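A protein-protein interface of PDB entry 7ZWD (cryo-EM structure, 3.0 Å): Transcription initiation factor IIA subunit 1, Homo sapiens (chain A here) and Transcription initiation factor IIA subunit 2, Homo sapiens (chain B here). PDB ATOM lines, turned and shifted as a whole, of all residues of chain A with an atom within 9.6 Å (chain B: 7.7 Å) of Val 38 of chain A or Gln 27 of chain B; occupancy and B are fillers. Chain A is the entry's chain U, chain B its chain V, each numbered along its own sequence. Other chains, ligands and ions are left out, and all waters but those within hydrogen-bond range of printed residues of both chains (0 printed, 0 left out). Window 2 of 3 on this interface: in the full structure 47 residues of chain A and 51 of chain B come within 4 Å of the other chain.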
ATOM      1  N   ILE A  22      -9.037  -0.460   3.365  1.00  0.00           N
ATOM      2  CA  ILE A  22      -8.379   0.294   4.426  1.00  0.00           C
ATOM      3  C   ILE A  22      -7.858  -0.643   5.505  1.00  0.00           C
ATOM      4  O   ILE A  22      -6.753  -0.458   6.024  1.00  0.00           O
ATOM      5  CB  ILE A  22      -9.337   1.346   5.003  1.00  0.00           C
ATOM      6  CG1 ILE A  22      -9.502   2.493   4.008  1.00  0.00           C
ATOM      7  CG2 ILE A  22      -8.844   1.840   6.346  1.00  0.00           C
ATOM      8  CD1 ILE A  22      -8.197   3.038   3.487  1.00  0.00           C
ATOM      9  N   VAL A  25      -4.569  -2.583   4.110  1.00  0.00           N
ATOM     10  CA  VAL A  25      -3.338  -1.848   3.853  1.00  0.00           C
ATOM     11  C   VAL A  25      -2.847  -1.092   5.073  1.00  0.00           C
ATOM     12  O   VAL A  25      -1.807  -0.425   4.997  1.00  0.00           O
ATOM     13  CB  VAL A  25      -3.506  -0.863   2.682  1.00  0.00           C
ATOM     14  CG1 VAL A  25      -4.118  -1.568   1.496  1.00  0.00           C
ATOM     15  CG2 VAL A  25      -4.348   0.318   3.106  1.00  0.00           C
ATOM     16  N   ARG A  26      -3.561  -1.170   6.195  1.00  0.00           N
ATOM     17  CA  ARG A  26      -3.126  -0.482   7.405  1.00  0.00           C
ATOM     18  C   ARG A  26      -1.705  -0.874   7.781  1.00  0.00           C
ATOM     19  O   ARG A  26      -0.894  -0.024   8.173  1.00  0.00           O
ATOM     20  CB  ARG A  26      -4.088  -0.799   8.543  1.00  0.00           C
ATOM     21  CG  ARG A  26      -3.710  -0.210   9.870  1.00  0.00           C
ATOM     22  CD  ARG A  26      -4.895  -0.268  10.801  1.00  0.00           C
ATOM     23  NE  ARG A  26      -6.040   0.438  10.239  1.00  0.00           N
ATOM     24  CZ  ARG A  26      -7.302   0.194  10.568  1.00  0.00           C
ATOM     25  NH1 ARG A  26      -7.587  -0.748  11.455  1.00  0.00           N
ATOM     26  NH2 ARG A  26      -8.280   0.889  10.009  1.00  0.00           N
ATOM     27  N   PHE A  29       1.021   0.786   5.592  1.00  0.00           N
ATOM     28  CA  PHE A  29       1.197   2.174   5.993  1.00  0.00           C
ATOM     29  C   PHE A  29       2.000   2.263   7.281  1.00  0.00           C
ATOM     30  O   PHE A  29       2.905   3.096   7.409  1.00  0.00           O
ATOM     31  CB  PHE A  29      -0.165   2.844   6.156  1.00  0.00           C
ATOM     32  CG  PHE A  29      -0.786   3.276   4.864  1.00  0.00           C
ATOM     33  CD1 PHE A  29      -1.027   2.362   3.857  1.00  0.00           C
ATOM     34  CD2 PHE A  29      -1.144   4.593   4.663  1.00  0.00           C
ATOM     35  CE1 PHE A  29      -1.604   2.753   2.672  1.00  0.00           C
ATOM     36  CE2 PHE A  29      -1.721   4.992   3.479  1.00  0.00           C
ATOM     37  CZ  PHE A  29      -1.951   4.070   2.483  1.00  0.00           C
ATOM     38  N   LEU A  30       1.683   1.402   8.249  1.00  0.00           N
ATOM     39  CA  LEU A  30       2.484   1.331   9.466  1.00  0.00           C
ATOM     40  C   LEU A  30       3.937   0.990   9.154  1.00  0.00           C
ATOM     41  O   LEU A  30       4.857   1.565   9.746  1.00  0.00           O
ATOM     42  CB  LEU A  30       1.875   0.301  10.418  1.00  0.00           C
ATOM     43  CG  LEU A  30       2.687  -0.216  11.607  1.00  0.00           C
ATOM     44  CD1 LEU A  30       1.761  -0.515  12.767  1.00  0.00           C
ATOM     45  CD2 LEU A  30       3.456  -1.477  11.235  1.00  0.00           C
ATOM     46  N   ASP A  32       6.004   1.030   6.127  1.00  0.00           N
ATOM     47  CA  ASP A  32       6.885   1.925   5.389  1.00  0.00           C
ATOM     48  C   ASP A  32       7.082   3.263   6.085  1.00  0.00           C
ATOM     49  O   ASP A  32       7.910   4.061   5.632  1.00  0.00           O
ATOM     50  CB  ASP A  32       6.357   2.157   3.975  1.00  0.00           C
ATOM     51  CG  ASP A  32       5.051   2.910   3.960  1.00  0.00           C
ATOM     52  OD1 ASP A  32       4.406   3.015   5.024  1.00  0.00           O
ATOM     53  OD2 ASP A  32       4.680   3.413   2.881  1.00  0.00           O
ATOM     54  N   GLY A  33       6.344   3.533   7.152  1.00  0.00           N
ATOM     55  CA  GLY A  33       6.562   4.705   7.959  1.00  0.00           C
ATOM     56  C   GLY A  33       5.689   5.894   7.647  1.00  0.00           C
ATOM     57  O   GLY A  33       6.173   7.028   7.726  1.00  0.00           O
ATOM     58  N   VAL A  34       4.425   5.681   7.297  1.00  0.00           N
ATOM     59  CA  VAL A  34       3.476   6.767   7.087  1.00  0.00           C
ATOM     60  C   VAL A  34       2.370   6.603   8.118  1.00  0.00           C
ATOM     61  O   VAL A  34       1.819   5.507   8.280  1.00  0.00           O
ATOM     62  CB  VAL A  34       2.916   6.793   5.657  1.00  0.00           C
ATOM     63  CG1 VAL A  34       2.317   5.458   5.277  1.00  0.00           C
ATOM     64  CG2 VAL A  34       1.891   7.898   5.514  1.00  0.00           C
ATOM     65  N   ASP A  35       2.061   7.683   8.835  1.00  0.00           N
ATOM     66  CA  ASP A  35       1.130   7.635   9.954  1.00  0.00           C
ATOM     67  C   ASP A  35      -0.249   7.155   9.526  1.00  0.00           C
ATOM     68  O   ASP A  35      -0.631   7.297   8.361  1.00  0.00           O
ATOM     69  CB  ASP A  35       1.030   9.013  10.610  1.00  0.00           C
ATOM     70  CG  ASP A  35       0.550  10.083   9.648  1.00  0.00           C
ATOM     71  OD1 ASP A  35       1.355  10.970   9.299  1.00  0.00           O
ATOM     72  OD2 ASP A  35      -0.630  10.046   9.242  1.00  0.00           O
ATOM     73  N   GLU A  36      -1.003   6.588  10.467  1.00  0.00           N
ATOM     74  CA  GLU A  36      -2.348   6.125  10.162  1.00  0.00           C
ATOM     75  C   GLU A  36      -3.325   7.274   9.970  1.00  0.00           C
ATOM     76  O   GLU A  36      -4.427   7.057   9.457  1.00  0.00           O
ATOM     77  CB  GLU A  36      -2.837   5.189  11.266  1.00  0.00           C
ATOM     78  CG  GLU A  36      -2.427   3.738  11.064  1.00  0.00           C
ATOM     79  CD  GLU A  36      -0.920   3.546  11.036  1.00  0.00           C
ATOM     80  OE1 GLU A  36      -0.199   4.365  11.644  1.00  0.00           O
ATOM     81  OE2 GLU A  36      -0.454   2.576  10.401  1.00  0.00           O
ATOM     82  N   GLN A  37      -2.956   8.490  10.374  1.00  0.00           N
ATOM     83  CA  GLN A  37      -3.791   9.636  10.044  1.00  0.00           C
ATOM     84  C   GLN A  37      -3.850   9.847   8.543  1.00  0.00           C
ATOM     85  O   GLN A  37      -4.894  10.235   8.013  1.00  0.00           O
ATOM     86  CB  GLN A  37      -3.277  10.887  10.750  1.00  0.00           C
ATOM     87  CG  GLN A  37      -3.302  10.759  12.253  1.00  0.00           C
ATOM     88  CD  GLN A  37      -4.563  10.078  12.739  1.00  0.00           C
ATOM     89  OE1 GLN A  37      -5.663  10.608  12.590  1.00  0.00           O
ATOM     90  NE2 GLN A  37      -4.411   8.890  13.309  1.00  0.00           N
ATOM     91  N   VAL A  38      -2.749   9.581   7.839  1.00  0.00           N
ATOM     92  CA  VAL A  38      -2.786   9.585   6.381  1.00  0.00           C
ATOM     93  C   VAL A  38      -3.738   8.511   5.878  1.00  0.00           C
ATOM     94  O   VAL A  38      -4.435   8.698   4.876  1.00  0.00           O
ATOM     95  CB  VAL A  38      -1.367   9.406   5.810  1.00  0.00           C
ATOM     96  CG1 VAL A  38      -1.423   8.966   4.361  1.00  0.00           C
ATOM     97  CG2 VAL A  38      -0.582  10.698   5.939  1.00  0.00           C
ATOM     98  N   LEU A  39      -3.806   7.381   6.580  1.00  0.00           N
ATOM     99  CA  LEU A  39      -4.721   6.322   6.174  1.00  0.00           C
ATOM    100  C   LEU A  39      -6.172   6.758   6.323  1.00  0.00           C
ATOM    101  O   LEU A  39      -6.988   6.545   5.419  1.00  0.00           O
ATOM    102  CB  LEU A  39      -4.455   5.065   6.996  1.00  0.00           C
ATOM    103  CG  LEU A  39      -5.248   3.836   6.581  1.00  0.00           C
ATOM    104  CD1 LEU A  39      -4.808   3.396   5.205  1.00  0.00           C
ATOM    105  CD2 LEU A  39      -5.046   2.727   7.589  1.00  0.00           C
ATOM    106  N   MET A  40      -6.512   7.370   7.457  1.00  0.00           N
ATOM    107  CA  MET A  40      -7.873   7.861   7.640  1.00  0.00           C
ATOM    108  C   MET A  40      -8.185   8.985   6.664  1.00  0.00           C
ATOM    109  O   MET A  40      -9.321   9.110   6.192  1.00  0.00           O
ATOM    110  CB  MET A  40      -8.077   8.326   9.079  1.00  0.00           C
ATOM    111  CG  MET A  40      -8.098   7.226  10.144  1.00  0.00           C
ATOM    112  SD  MET A  40      -9.079   5.749   9.786  1.00  0.00           S
ATOM    113  CE  MET A  40      -7.906   4.702   8.929  1.00  0.00           C
ATOM    114  N   GLU A  41      -7.192   9.815   6.352  1.00  0.00           N
ATOM    115  CA  GLU A  41      -7.378  10.842   5.336  1.00  0.00           C
ATOM    116  C   GLU A  41      -7.694  10.215   3.990  1.00  0.00           C
ATOM    117  O   GLU A  41      -8.585  10.674   3.272  1.00  0.00           O
ATOM    118  CB  GLU A  41      -6.130  11.717   5.243  1.00  0.00           C
ATOM    119  CG  GLU A  41      -6.200  12.775   4.159  1.00  0.00           C
ATOM    120  CD  GLU A  41      -4.835  13.135   3.613  1.00  0.00           C
ATOM    121  OE1 GLU A  41      -3.856  12.440   3.957  1.00  0.00           O
ATOM    122  OE2 GLU A  41      -4.738  14.116   2.844  1.00  0.00           O
ATOM    123  N   LEU A  42      -6.963   9.161   3.632  1.00  0.00           N
ATOM    124  CA  LEU A  42      -7.262   8.418   2.415  1.00  0.00           C
ATOM    125  C   LEU A  42      -8.688   7.898   2.432  1.00  0.00           C
ATOM    126  O   LEU A  42      -9.411   8.002   1.438  1.00  0.00           O
ATOM    127  CB  LEU A  42      -6.281   7.260   2.259  1.00  0.00           C
ATOM    128  CG  LEU A  42      -6.736   6.131   1.333  1.00  0.00           C
ATOM    129  CD1 LEU A  42      -6.845   6.604  -0.103  1.00  0.00           C
ATOM    130  CD2 LEU A  42      -5.796   4.945   1.441  1.00  0.00           C
ATOM    131  N   LYS A  43      -9.107   7.323   3.556  1.00  0.00           N
ATOM    132  CA  LYS A  43     -10.440   6.737   3.626  1.00  0.00           C
ATOM    133  C   LYS A  43     -11.516   7.798   3.434  1.00  0.00           C
ATOM    134  O   LYS A  43     -12.448   7.619   2.639  1.00  0.00           O
ATOM    135  CB  LYS A  43     -10.623   6.012   4.955  1.00  0.00           C
ATOM    136  CG  LYS A  43     -11.823   5.091   4.989  1.00  0.00           C
ATOM    137  CD  LYS A  43     -12.927   5.662   5.843  1.00  0.00           C
ATOM    138  CE  LYS A  43     -14.095   4.704   5.929  1.00  0.00           C
ATOM    139  NZ  LYS A  43     -15.180   5.240   6.793  1.00  0.00           N
ATOM    140  N   THR A  44     -11.403   8.920   4.147  1.00  0.00           N
ATOM    141  CA  THR A  44     -12.412   9.966   4.012  1.00  0.00           C
ATOM    142  C   THR A  44     -12.365  10.600   2.632  1.00  0.00           C
ATOM    143  O   THR A  44     -13.408  10.927   2.059  1.00  0.00           O
ATOM    144  CB  THR A  44     -12.240  11.039   5.082  1.00  0.00           C
ATOM    145  OG1 THR A  44     -11.110  11.858   4.762  1.00  0.00           O
ATOM    146  CG2 THR A  44     -12.073  10.418   6.454  1.00  0.00           C
ATOM    147  N   LEU A  45     -11.168  10.779   2.078  1.00  0.00           N
ATOM    148  CA  LEU A  45     -11.055  11.350   0.745  1.00  0.00           C
ATOM    149  C   LEU A  45     -11.700  10.443  -0.289  1.00  0.00           C
ATOM    150  O   LEU A  45     -12.377  10.915  -1.205  1.00  0.00           O
ATOM    151  CB  LEU A  45      -9.584  11.585   0.416  1.00  0.00           C
ATOM    152  CG  LEU A  45      -9.284  12.328  -0.877  1.00  0.00           C
ATOM    153  CD1 LEU A  45     -10.140  13.576  -0.980  1.00  0.00           C
ATOM    154  CD2 LEU A  45      -7.813  12.677  -0.924  1.00  0.00           C
ATOM    155  N   TRP A  46     -11.507   9.134  -0.148  1.00  0.00           N
ATOM    156  CA  TRP A  46     -12.146   8.172  -1.033  1.00  0.00           C
ATOM    157  C   TRP A  46     -13.658   8.238  -0.904  1.00  0.00           C
ATOM    158  O   TRP A  46     -14.379   8.324  -1.905  1.00  0.00           O
ATOM    159  CB  TRP A  46     -11.642   6.775  -0.697  1.00  0.00           C
ATOM    160  CG  TRP A  46     -11.816   5.795  -1.770  1.00  0.00           C
ATOM    161  CD1 TRP A  46     -12.277   6.030  -3.021  1.00  0.00           C
ATOM    162  CD2 TRP A  46     -11.516   4.403  -1.702  1.00  0.00           C
ATOM    163  NE1 TRP A  46     -12.292   4.864  -3.745  1.00  0.00           N
ATOM    164  CE2 TRP A  46     -11.828   3.849  -2.952  1.00  0.00           C
ATOM    165  CE3 TRP A  46     -11.017   3.570  -0.701  1.00  0.00           C
ATOM    166  CZ2 TRP A  46     -11.656   2.504  -3.230  1.00  0.00           C
ATOM    167  CZ3 TRP A  46     -10.848   2.238  -0.976  1.00  0.00           C
ATOM    168  CH2 TRP A  46     -11.166   1.714  -2.229  1.00  0.00           C
ATOM    169  N   SER B  18      -7.925   9.718  -5.642  1.00  0.00           N
ATOM    170  CA  SER B  18      -7.520   9.978  -4.266  1.00  0.00           C
ATOM    171  C   SER B  18      -6.038   9.691  -4.073  1.00  0.00           C
ATOM    172  O   SER B  18      -5.324  10.452  -3.411  1.00  0.00           O
ATOM    173  CB  SER B  18      -8.360   9.141  -3.305  1.00  0.00           C
ATOM    174  OG  SER B  18      -7.713   9.017  -2.055  1.00  0.00           O
ATOM    175  N   GLU B  21      -4.121  12.504  -5.550  1.00  0.00           N
ATOM    176  CA  GLU B  21      -4.142  13.663  -4.666  1.00  0.00           C
ATOM    177  C   GLU B  21      -3.176  13.480  -3.504  1.00  0.00           C
ATOM    178  O   GLU B  21      -2.533  14.439  -3.063  1.00  0.00           O
ATOM    179  CB  GLU B  21      -5.558  13.904  -4.147  1.00  0.00           C
ATOM    180  CG  GLU B  21      -6.403  14.796  -5.036  1.00  0.00           C
ATOM    181  CD  GLU B  21      -7.741  15.133  -4.413  1.00  0.00           C
ATOM    182  OE1 GLU B  21      -8.712  15.350  -5.166  1.00  0.00           O
ATOM    183  OE2 GLU B  21      -7.824  15.182  -3.167  1.00  0.00           O
ATOM    184  N   LEU B  22      -3.062  12.253  -2.996  1.00  0.00           N
ATOM    185  CA  LEU B  22      -2.133  11.999  -1.901  1.00  0.00           C
ATOM    186  C   LEU B  22      -0.686  12.044  -2.370  1.00  0.00           C
ATOM    187  O   LEU B  22       0.198  12.458  -1.611  1.00  0.00           O
ATOM    188  CB  LEU B  22      -2.435  10.649  -1.258  1.00  0.00           C
ATOM    189  CG  LEU B  22      -3.559  10.671  -0.230  1.00  0.00           C
ATOM    190  CD1 LEU B  22      -3.549   9.403   0.592  1.00  0.00           C
ATOM    191  CD2 LEU B  22      -3.425  11.889   0.656  1.00  0.00           C
ATOM    192  N   ILE B  23      -0.424  11.620  -3.605  1.00  0.00           N
ATOM    193  CA  ILE B  23       0.940  11.625  -4.120  1.00  0.00           C
ATOM    194  C   ILE B  23       1.392  13.049  -4.411  1.00  0.00           C
ATOM    195  O   ILE B  23       2.477  13.469  -3.996  1.00  0.00           O
ATOM    196  CB  ILE B  23       1.044  10.739  -5.371  1.00  0.00           C
ATOM    197  CG1 ILE B  23       1.043   9.265  -4.983  1.00  0.00           C
ATOM    198  CG2 ILE B  23       2.296  11.078  -6.157  1.00  0.00           C
ATOM    199  CD1 ILE B  23       1.090   8.333  -6.163  1.00  0.00           C
ATOM    200  N   GLN B  24       0.568  13.811  -5.133  1.00  0.00           N
ATOM    201  CA  GLN B  24       0.924  15.190  -5.439  1.00  0.00           C
ATOM    202  C   GLN B  24       1.063  16.032  -4.180  1.00  0.00           C
ATOM    203  O   GLN B  24       1.749  17.058  -4.206  1.00  0.00           O
ATOM    204  CB  GLN B  24      -0.115  15.814  -6.370  1.00  0.00           C
ATOM    205  CG  GLN B  24      -1.458  16.072  -5.715  1.00  0.00           C
ATOM    206  CD  GLN B  24      -2.583  16.187  -6.719  1.00  0.00           C
ATOM    207  OE1 GLN B  24      -2.966  15.207  -7.356  1.00  0.00           O
ATOM    208  NE2 GLN B  24      -3.119  17.392  -6.868  1.00  0.00           N
ATOM    209  N   SER B  25       0.427  15.626  -3.087  1.00  0.00           N
ATOM    210  CA  SER B  25       0.600  16.275  -1.798  1.00  0.00           C
ATOM    211  C   SER B  25       1.792  15.729  -1.027  1.00  0.00           C
ATOM    212  O   SER B  25       1.989  16.109   0.133  1.00  0.00           O
ATOM    213  CB  SER B  25      -0.674  16.127  -0.963  1.00  0.00           C
ATOM    214  OG  SER B  25      -0.686  14.889  -0.280  1.00  0.00           O
ATOM    215  N   GLN B  26       2.580  14.844  -1.642  1.00  0.00           N
ATOM    216  CA  GLN B  26       3.824  14.337  -1.061  1.00  0.00           C
ATOM    217  C   GLN B  26       3.583  13.683   0.295  1.00  0.00           C
ATOM    218  O   GLN B  26       4.394  13.799   1.215  1.00  0.00           O
ATOM    219  CB  GLN B  26       4.874  15.444  -0.951  1.00  0.00           C
ATOM    220  CG  GLN B  26       5.402  15.923  -2.292  1.00  0.00           C
ATOM    221  CD  GLN B  26       4.482  16.929  -2.951  1.00  0.00           C
ATOM    222  OE1 GLN B  26       3.799  17.700  -2.275  1.00  0.00           O
ATOM    223  NE2 GLN B  26       4.448  16.920  -4.277  1.00  0.00           N
ATOM    224  N   GLN B  27       2.460  12.986   0.420  1.00  0.00           N
ATOM    225  CA  GLN B  27       2.119  12.293   1.650  1.00  0.00           C
ATOM    226  C   GLN B  27       2.240  10.784   1.530  1.00  0.00           C
ATOM    227  O   GLN B  27       1.939  10.074   2.496  1.00  0.00           O
ATOM    228  CB  GLN B  27       0.700  12.663   2.090  1.00  0.00           C
ATOM    229  CG  GLN B  27       0.534  14.120   2.473  1.00  0.00           C
ATOM    230  CD  GLN B  27      -0.789  14.393   3.159  1.00  0.00           C
ATOM    231  OE1 GLN B  27      -0.967  14.080   4.335  1.00  0.00           O
ATOM    232  NE2 GLN B  27      -1.725  14.981   2.426  1.00  0.00           N
ATOM    233  N   ILE B  28       2.683  10.274   0.382  1.00  0.00           N
ATOM    234  CA  ILE B  28       2.699   8.840   0.131  1.00  0.00           C
ATOM    235  C   ILE B  28       3.590   8.570  -1.072  1.00  0.00           C
ATOM    236  O   ILE B  28       3.815   9.446  -1.909  1.00  0.00           O
ATOM    237  CB  ILE B  28       1.263   8.305  -0.085  1.00  0.00           C
ATOM    238  CG1 ILE B  28       1.179   6.821   0.247  1.00  0.00           C
ATOM    239  CG2 ILE B  28       0.799   8.566  -1.502  1.00  0.00           C
ATOM    240  CD1 ILE B  28      -0.236   6.316   0.323  1.00  0.00           C
ATOM    241  N   THR B  29       4.116   7.343  -1.145  1.00  0.00           N
ATOM    242  CA  THR B  29       4.993   6.973  -2.245  1.00  0.00           C
ATOM    243  C   THR B  29       4.230   6.192  -3.311  1.00  0.00           C
ATOM    244  O   THR B  29       3.265   5.486  -3.003  1.00  0.00           O
ATOM    245  CB  THR B  29       6.166   6.138  -1.734  1.00  0.00           C
ATOM    246  OG1 THR B  29       7.076   5.872  -2.808  1.00  0.00           O
ATOM    247  CG2 THR B  29       5.685   4.823  -1.155  1.00  0.00           C
ATOM    248  N   LEU B  32       3.801   2.366  -2.479  1.00  0.00           N
ATOM    249  CA  LEU B  32       2.656   2.064  -1.632  1.00  0.00           C
ATOM    250  C   LEU B  32       1.353   2.290  -2.383  1.00  0.00           C
ATOM    251  O   LEU B  32       0.379   1.562  -2.180  1.00  0.00           O
ATOM    252  CB  LEU B  32       2.706   2.909  -0.359  1.00  0.00           C
ATOM    253  CG  LEU B  32       1.503   2.845   0.583  1.00  0.00           C
ATOM    254  CD1 LEU B  32       1.179   1.415   0.944  1.00  0.00           C
ATOM    255  CD2 LEU B  32       1.757   3.654   1.834  1.00  0.00           C
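Hydrophobic or aromatic side chains of chain B within 4 Å of the printed part of chain A: Leu 22, Ile 28 and Leu 32.
Hydrophobic or aromatic side chains of chain A within 4 Å of the printed part of chain B: Phe 29, Val 34, Val 38, Leu 42 and Leu 45.
Along chain A the printed residues that touch a printed residue of chain B span positions 29 to 45.
The backbone NH (N) of Val 34 of chain A lies within hydrogen-bond range of the backbone carbonyl oxygen (O) of Phe 29 of chain A (3.0 Å).
The backbone carbonyl oxygen (O) of Glu 41 of chain A is in hydrogen-bond range of the side-chain hydroxyl (OG1) of Thr 44 of chain A.
OE1 of Gln 24 of chain B sits close to N of Glu 21 of chain B (3.4 Å).
The backbone carbonyl oxygen (O) of Leu 22 of chain B is in hydrogen-bond range of the side-chain hydroxyl (OG) of Ser 25 of chain B (2.9 Å).
The backbone carbonyl oxygen (O) of Leu 22 of chain B lies within hydrogen-bond range of the backbone NH (N) of Gln 27 of chain B.
The side-chain hydroxyl (OG) of Ser 25 of chain B lies within hydrogen-bond range of the side-chain amide nitrogen (NE2) of Gln 27 of chain B (2.9 Å).
The side-chain carboxylate (OE2) of Glu 41 of chain A lies within hydrogen-bond range of the side-chain amide nitrogen (NE2) of Gln 27 of chain B.
Phe 29 of chain A touches Ile 28 of chain B.
CD1 of Leu 32 of chain B touches CE1 of Phe 29 of chain A (3.5 Å).
Asp 32 of chain A touches Leu 32 of chain B (OD2 to CD2, 3.1 Å).
Gln 27 of chain B touches Val 34 of chain A.
CD2 of Leu 32 of chain B touches CG1 of Val 34 of chain A, 3.9 Å away.
CG2 of Val 38 of chain A touches OE1 of Gln 27 of chain B (3.8 Å).
Leu 22 of chain B touches Glu 41 of chain A (CD2 to OE1, 3.4 Å).
CB of Leu 42 of chain A touches CD1 of Leu 22 of chain B, at 3.9 Å.
Leu 45 of chain A touches Ser 18 of chain B (CD2 to OG, 3.8 Å).
Glu 21 of chain B touches Leu 45 of chain A (OE2 to CD2, 3.4 Å).
Of chain B, only Gln 27 (3.8 Å) comes within 4 Å of Val 38 of chain A.
Of chain A, only Val 34 (3.7 Å), Val 38 (3.8 Å) and Glu 41 (3.2 Å) come within 4 Å of Gln 27 of chain B.
No residue of chain A comes within 4 Å of Ser 25 of chain B.
Of the printed residues of chain A, Ile 28 of chain B touches Phe 29.
Of the printed residues of chain A, Leu 22 of chain B touches Glu 41 and Leu 42.
Of the printed residues of chain B, Glu 41 of chain A touches Leu 22 and Gln 27.
Printed residues of chain B within 4 Å of Val 34 of chain A: Gln 27 and Leu 32.
Gln 24 of chain B touches none of the printed residues of chain A.
Thr 44 of chain A touches none of the printed residues of chain B.
The nearest printed residue of chain B that does not touch Leu 45 of chain A is Leu 22 of chain B (4.7 Å).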
